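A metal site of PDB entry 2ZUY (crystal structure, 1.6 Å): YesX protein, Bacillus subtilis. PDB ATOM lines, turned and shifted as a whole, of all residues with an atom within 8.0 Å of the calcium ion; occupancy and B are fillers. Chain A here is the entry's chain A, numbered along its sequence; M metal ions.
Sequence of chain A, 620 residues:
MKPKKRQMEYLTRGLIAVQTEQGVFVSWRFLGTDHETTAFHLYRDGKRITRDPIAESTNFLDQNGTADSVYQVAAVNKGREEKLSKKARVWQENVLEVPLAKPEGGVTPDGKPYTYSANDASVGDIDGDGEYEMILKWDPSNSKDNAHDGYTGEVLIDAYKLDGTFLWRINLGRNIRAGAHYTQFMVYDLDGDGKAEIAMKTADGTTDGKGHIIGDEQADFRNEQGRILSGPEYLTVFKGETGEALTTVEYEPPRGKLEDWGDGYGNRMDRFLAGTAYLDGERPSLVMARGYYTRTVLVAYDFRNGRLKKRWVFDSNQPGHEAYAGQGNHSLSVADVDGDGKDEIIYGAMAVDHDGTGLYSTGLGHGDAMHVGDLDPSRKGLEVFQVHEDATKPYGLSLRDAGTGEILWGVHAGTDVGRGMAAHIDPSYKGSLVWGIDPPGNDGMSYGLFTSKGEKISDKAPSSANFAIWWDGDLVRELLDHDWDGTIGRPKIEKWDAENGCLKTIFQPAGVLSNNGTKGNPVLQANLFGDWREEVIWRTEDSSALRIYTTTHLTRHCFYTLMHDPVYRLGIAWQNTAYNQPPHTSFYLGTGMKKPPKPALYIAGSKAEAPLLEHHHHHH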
ATOM      1  N   GLN A   7     -27.975  15.245  19.873  1.00  0.00           N
ATOM      2  CA  GLN A   7     -26.717  14.516  19.895  1.00  0.00           C
ATOM      3  C   GLN A   7     -25.836  15.079  21.004  1.00  0.00           C
ATOM      4  O   GLN A   7     -25.633  16.289  21.068  1.00  0.00           O
ATOM      5  CB  GLN A   7     -26.005  14.659  18.549  1.00  0.00           C
ATOM      6  CG  GLN A   7     -24.601  14.069  18.522  1.00  0.00           C
ATOM      7  CD  GLN A   7     -23.738  14.658  17.422  1.00  0.00           C
ATOM      8  OE1 GLN A   7     -24.095  14.599  16.242  1.00  0.00           O
ATOM      9  NE2 GLN A   7     -22.591  15.225  17.811  1.00  0.00           N
ATOM     10  N   ASP A 125     -13.612  15.293  23.102  1.00  0.00           N
ATOM     11  CA  ASP A 125     -13.158  13.916  23.220  1.00  0.00           C
ATOM     12  C   ASP A 125     -12.736  13.472  21.825  1.00  0.00           C
ATOM     13  O   ASP A 125     -13.568  13.142  20.984  1.00  0.00           O
ATOM     14  CB  ASP A 125     -14.280  13.043  23.761  1.00  0.00           C
ATOM     15  CG  ASP A 125     -13.868  11.588  23.918  1.00  0.00           C
ATOM     16  OD1 ASP A 125     -12.675  11.257  23.747  1.00  0.00           O
ATOM     17  OD2 ASP A 125     -14.773  10.765  24.199  1.00  0.00           O
ATOM     18  N   ILE A 126     -11.436  13.511  21.572  1.00  0.00           N
ATOM     19  CA  ILE A 126     -10.947  13.315  20.205  1.00  0.00           C
ATOM     20  C   ILE A 126     -10.850  11.849  19.779  1.00  0.00           C
ATOM     21  O   ILE A 126     -10.760  11.558  18.580  1.00  0.00           O
ATOM     22  CB  ILE A 126      -9.636  14.107  19.924  1.00  0.00           C
ATOM     23  CG1 ILE A 126      -8.519  13.788  20.925  1.00  0.00           C
ATOM     24  CG2 ILE A 126      -9.912  15.604  19.998  1.00  0.00           C
ATOM     25  CD1 ILE A 126      -7.871  12.434  20.760  1.00  0.00           C
ATOM     26  N   TYR A 188     -15.687  20.327  18.453  1.00  0.00           N
ATOM     27  CA  TYR A 188     -16.971  19.657  18.617  1.00  0.00           C
ATOM     28  C   TYR A 188     -17.030  18.429  17.730  1.00  0.00           C
ATOM     29  O   TYR A 188     -16.362  18.373  16.690  1.00  0.00           O
ATOM     30  CB  TYR A 188     -18.124  20.610  18.263  1.00  0.00           C
ATOM     31  CG  TYR A 188     -19.374  20.334  19.093  1.00  0.00           C
ATOM     32  CD1 TYR A 188     -19.515  20.888  20.365  1.00  0.00           C
ATOM     33  CD2 TYR A 188     -20.405  19.515  18.612  1.00  0.00           C
ATOM     34  CE1 TYR A 188     -20.633  20.642  21.137  1.00  0.00           C
ATOM     35  CE2 TYR A 188     -21.539  19.265  19.384  1.00  0.00           C
ATOM     36  CZ  TYR A 188     -21.640  19.822  20.657  1.00  0.00           C
ATOM     37  OH  TYR A 188     -22.751  19.598  21.436  1.00  0.00           O
ATOM     38  N   ASP A 189     -17.834  17.449  18.131  1.00  0.00           N
ATOM     39  CA  ASP A 189     -18.122  16.322  17.252  1.00  0.00           C
ATOM     40  C   ASP A 189     -19.228  16.761  16.295  1.00  0.00           C
ATOM     41  O   ASP A 189     -20.419  16.574  16.563  1.00  0.00           O
ATOM     42  CB  ASP A 189     -18.518  15.089  18.072  1.00  0.00           C
ATOM     43  CG  ASP A 189     -18.842  13.889  17.212  1.00  0.00           C
ATOM     44  OD1 ASP A 189     -18.507  13.902  16.006  1.00  0.00           O
ATOM     45  OD2 ASP A 189     -19.440  12.923  17.755  1.00  0.00           O
ATOM     46  N   LEU A 190     -18.821  17.369  15.181  1.00  0.00           N
ATOM     47  CA  LEU A 190     -19.776  17.956  14.246  1.00  0.00           C
ATOM     48  C   LEU A 190     -20.584  16.944  13.430  1.00  0.00           C
ATOM     49  O   LEU A 190     -21.720  17.223  13.057  1.00  0.00           O
ATOM     50  CB  LEU A 190     -19.096  18.964  13.297  1.00  0.00           C
ATOM     51  CG  LEU A 190     -18.465  20.180  13.977  1.00  0.00           C
ATOM     52  CD1 LEU A 190     -17.561  20.942  13.002  1.00  0.00           C
ATOM     53  CD2 LEU A 190     -19.533  21.099  14.580  1.00  0.00           C
ATOM     54  N   ASP A 191     -19.970  15.793  13.139  1.00  0.00           N
ATOM     55  CA  ASP A 191     -20.629  14.787  12.285  1.00  0.00           C
ATOM     56  C   ASP A 191     -21.276  13.629  13.064  1.00  0.00           C
ATOM     57  O   ASP A 191     -21.993  12.807  12.494  1.00  0.00           O
ATOM     58  CB  ASP A 191     -19.667  14.258  11.218  1.00  0.00           C
ATOM     59  CG  ASP A 191     -18.468  13.535  11.805  1.00  0.00           C
ATOM     60  OD1 ASP A 191     -18.324  13.484  13.054  1.00  0.00           O
ATOM     61  OD2 ASP A 191     -17.645  13.019  11.016  1.00  0.00           O
ATOM     62  N   GLY A 192     -21.011  13.583  14.374  1.00  0.00           N
ATOM     63  CA  GLY A 192     -21.661  12.608  15.254  1.00  0.00           C
ATOM     64  C   GLY A 192     -21.093  11.194  15.262  1.00  0.00           C
ATOM     65  O   GLY A 192     -21.793  10.241  15.611  1.00  0.00           O
ATOM     66  N   ASP A 193     -19.818  11.046  14.885  1.00  0.00           N
ATOM     67  CA  ASP A 193     -19.148   9.738  14.947  1.00  0.00           C
ATOM     68  C   ASP A 193     -18.613   9.393  16.353  1.00  0.00           C
ATOM     69  O   ASP A 193     -18.136   8.278  16.582  1.00  0.00           O
ATOM     70  CB  ASP A 193     -18.019   9.652  13.901  1.00  0.00           C
ATOM     71  CG  ASP A 193     -16.753  10.375  14.324  1.00  0.00           C
ATOM     72  OD1 ASP A 193     -16.840  11.412  15.012  1.00  0.00           O
ATOM     73  OD2 ASP A 193     -15.653   9.930  13.936  1.00  0.00           O
ATOM     74  N   GLY A 194     -18.729  10.341  17.286  1.00  0.00           N
ATOM     75  CA  GLY A 194     -18.261  10.148  18.650  1.00  0.00           C
ATOM     76  C   GLY A 194     -16.890  10.760  18.955  1.00  0.00           C
ATOM     77  O   GLY A 194     -16.394  10.656  20.087  1.00  0.00           O
ATOM     78  N   LYS A 195     -16.295  11.405  17.960  1.00  0.00           N
ATOM     79  CA  LYS A 195     -14.973  12.018  18.129  1.00  0.00           C
ATOM     80  C   LYS A 195     -15.024  13.476  17.701  1.00  0.00           C
ATOM     81  O   LYS A 195     -15.570  13.814  16.648  1.00  0.00           O
ATOM     82  CB  LYS A 195     -13.905  11.266  17.323  1.00  0.00           C
ATOM     83  CG  LYS A 195     -13.783   9.782  17.633  1.00  0.00           C
ATOM     84  CD  LYS A 195     -12.734   9.143  16.744  1.00  0.00           C
ATOM     85  CE  LYS A 195     -12.705   7.624  16.902  1.00  0.00           C
ATOM     86  NZ  LYS A 195     -11.553   7.048  16.152  1.00  0.00           N
ATOM     87  N   ALA A 196     -14.412  14.349  18.501  1.00  0.00           N
ATOM     88  CA  ALA A 196     -14.399  15.775  18.195  1.00  0.00           C
ATOM     89  C   ALA A 196     -13.436  16.094  17.051  1.00  0.00           C
ATOM     90  O   ALA A 196     -12.433  15.416  16.860  1.00  0.00           O
ATOM     91  CB  ALA A 196     -14.037  16.580  19.424  1.00  0.00           C
ATOM     92  N   GLU A 197     -13.802  17.112  16.279  1.00  0.00           N
ATOM     93  CA  GLU A 197     -12.875  17.732  15.337  1.00  0.00           C
ATOM     94  C   GLU A 197     -12.713  19.194  15.709  1.00  0.00           C
ATOM     95  O   GLU A 197     -13.381  19.693  16.622  1.00  0.00           O
ATOM     96  CB  GLU A 197     -13.341  17.556  13.882  1.00  0.00           C
ATOM     97  CG  GLU A 197     -14.837  17.539  13.676  1.00  0.00           C
ATOM     98  CD  GLU A 197     -15.443  16.156  13.935  1.00  0.00           C
ATOM     99  OE1 GLU A 197     -14.696  15.153  14.034  1.00  0.00           O
ATOM    100  OE2 GLU A 197     -16.676  16.068  14.033  1.00  0.00           O
ATOM    101  N   ILE A 198     -11.801  19.863  15.001  1.00  0.00           N
ATOM    102  CA  ILE A 198     -11.481  21.261  15.271  1.00  0.00           C
ATOM    103  C   ILE A 198     -11.605  22.059  13.979  1.00  0.00           C
ATOM    104  O   ILE A 198     -10.959  21.731  12.983  1.00  0.00           O
ATOM    105  CB  ILE A 198     -10.057  21.433  15.860  1.00  0.00           C
ATOM    106  CG1 ILE A 198      -9.878  20.607  17.139  1.00  0.00           C
ATOM    107  CG2 ILE A 198      -9.773  22.897  16.157  1.00  0.00           C
ATOM    108  CD1 ILE A 198      -9.358  19.207  16.919  1.00  0.00           C
ATOM    109  N   VAL A 237     -11.496  21.994   8.590  1.00  0.00           N
ATOM    110  CA  VAL A 237     -11.868  21.072   9.650  1.00  0.00           C
ATOM    111  C   VAL A 237     -10.735  20.062   9.812  1.00  0.00           C
ATOM    112  O   VAL A 237     -10.333  19.402   8.830  1.00  0.00           O
ATOM    113  CB  VAL A 237     -13.199  20.323   9.366  1.00  0.00           C
ATOM    114  CG1 VAL A 237     -13.563  19.443  10.569  1.00  0.00           C
ATOM    115  CG2 VAL A 237     -14.335  21.296   9.055  1.00  0.00           C
ATOM    116  N   PHE A 238     -10.213  19.960  11.037  1.00  0.00           N
ATOM    117  CA  PHE A 238      -9.067  19.107  11.379  1.00  0.00           C
ATOM    118  C   PHE A 238      -9.539  17.909  12.190  1.00  0.00           C
ATOM    119  O   PHE A 238     -10.379  18.053  13.092  1.00  0.00           O
ATOM    120  CB  PHE A 238      -8.031  19.877  12.206  1.00  0.00           C
ATOM    121  CG  PHE A 238      -7.367  21.009  11.477  1.00  0.00           C
ATOM    122  CD1 PHE A 238      -6.213  20.805  10.720  1.00  0.00           C
ATOM    123  CD2 PHE A 238      -7.868  22.305  11.583  1.00  0.00           C
ATOM    124  CE1 PHE A 238      -5.580  21.857  10.067  1.00  0.00           C
ATOM    125  CE2 PHE A 238      -7.245  23.376  10.923  1.00  0.00           C
ATOM    126  CZ  PHE A 238      -6.097  23.148  10.172  1.00  0.00           C
ATOM    127  N   LYS A 239      -8.996  16.735  11.890  1.00  0.00           N
ATOM    128  CA  LYS A 239      -9.288  15.516  12.665  1.00  0.00           C
ATOM    129  C   LYS A 239      -8.803  15.668  14.114  1.00  0.00           C
ATOM    130  O   LYS A 239      -7.670  16.077  14.350  1.00  0.00           O
ATOM    131  CB  LYS A 239      -8.636  14.294  12.007  1.00  0.00           C
ATOM    132  CG  LYS A 239      -8.986  12.989  12.701  1.00  0.00           C
ATOM    133  CD  LYS A 239      -8.533  11.776  11.894  1.00  0.00           C
ATOM    134  CE  LYS A 239      -8.685  10.491  12.729  1.00  0.00           C
ATOM    135  NZ  LYS A 239     -10.045  10.328  13.367  1.00  0.00           N
ATOM    136  N   GLY A 240      -9.668  15.337  15.069  1.00  0.00           N
ATOM    137  CA  GLY A 240      -9.334  15.451  16.484  1.00  0.00           C
ATOM    138  C   GLY A 240      -8.142  14.655  16.962  1.00  0.00           C
ATOM    139  O   GLY A 240      -7.307  15.172  17.721  1.00  0.00           O
ATOM    140  N   LEU A 246      -8.914  17.596   7.288  1.00  0.00           N
ATOM    141  CA  LEU A 246      -9.903  16.731   6.638  1.00  0.00           C
ATOM    142  C   LEU A 246     -10.476  17.389   5.385  1.00  0.00           C
ATOM    143  O   LEU A 246     -10.607  16.750   4.336  1.00  0.00           O
ATOM    144  CB  LEU A 246     -11.023  16.348   7.605  1.00  0.00           C
ATOM    145  CG  LEU A 246     -10.606  15.490   8.806  1.00  0.00           C
ATOM    146  CD1 LEU A 246     -11.757  15.411   9.792  1.00  0.00           C
ATOM    147  CD2 LEU A 246     -10.191  14.088   8.349  1.00  0.00           C
ATOM    148  N   PHE A 303     -21.218  19.540   8.842  1.00  0.00           N
ATOM    149  CA  PHE A 303     -20.083  18.690   8.503  1.00  0.00           C
ATOM    150  C   PHE A 303     -20.551  17.248   8.518  1.00  0.00           C
ATOM    151  O   PHE A 303     -21.087  16.765   9.525  1.00  0.00           O
ATOM    152  CB  PHE A 303     -18.938  18.913   9.508  1.00  0.00           C
ATOM    153  CG  PHE A 303     -17.702  18.077   9.238  1.00  0.00           C
ATOM    154  CD1 PHE A 303     -16.900  18.330   8.116  1.00  0.00           C
ATOM    155  CD2 PHE A 303     -17.330  17.068  10.123  1.00  0.00           C
ATOM    156  CE1 PHE A 303     -15.749  17.563   7.886  1.00  0.00           C
ATOM    157  CE2 PHE A 303     -16.182  16.296   9.886  1.00  0.00           C
ATOM    158  CZ  PHE A 303     -15.394  16.550   8.771  1.00  0.00           C
ATOM    159  N   ALA A 604     -23.779  10.196  20.758  1.00  0.00           N
ATOM    160  CA  ALA A 604     -23.148  10.045  19.439  1.00  0.00           C
ATOM    161  C   ALA A 604     -22.268   8.795  19.404  1.00  0.00           C
ATOM    162  O   ALA A 604     -21.516   8.510  20.351  1.00  0.00           O
ATOM    163  CB  ALA A 604     -22.327  11.277  19.093  1.00  0.00           C
HETATM  164 CA    CA M   1     -16.604  13.638  14.601  1.00  0.00          CA
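OD1 of Asp 193 binds the calcium ion (2.3 Å). O of Lys 195 is bound to the calcium ion, 2.3 Å away. OD1 of Asp 191 is bound to the calcium ion. The side-chain carboxylate (OD1) of Asp 189 is bound to the calcium ion (2.4 Å). The calcium ion is bound by the side-chain carboxylate (OE2) of Glu 197. OE1 of Glu 197 is bound to the calcium ion (2.5 Å). The calcium ion has six donor atoms within binding distance.
Five residues have an atom within 4 Å of the calcium ion: Asp 189, Asp 191, Asp 193, Lys 195 and Glu 197. The nearest printed residue that does not touch the calcium ion is Leu 190 (4.4 Å).
N of Glu 197 sits at hydrogen-bond distance from O of Tyr 188, 2.9 Å away. OD2 of Asp 189 sits at hydrogen-bond distance from N of Gly 194. O of Asp 189 is in hydrogen-bond range of NE2 of Gln 7. The side-chain carboxylate of Asp 189 sits close to the backbone NH of Gly 192 (3.0 Å). The backbone NH (N) of Leu 190 lies close to the side-chain carboxylate (OE2) of Glu 197, at 2.8 Å.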
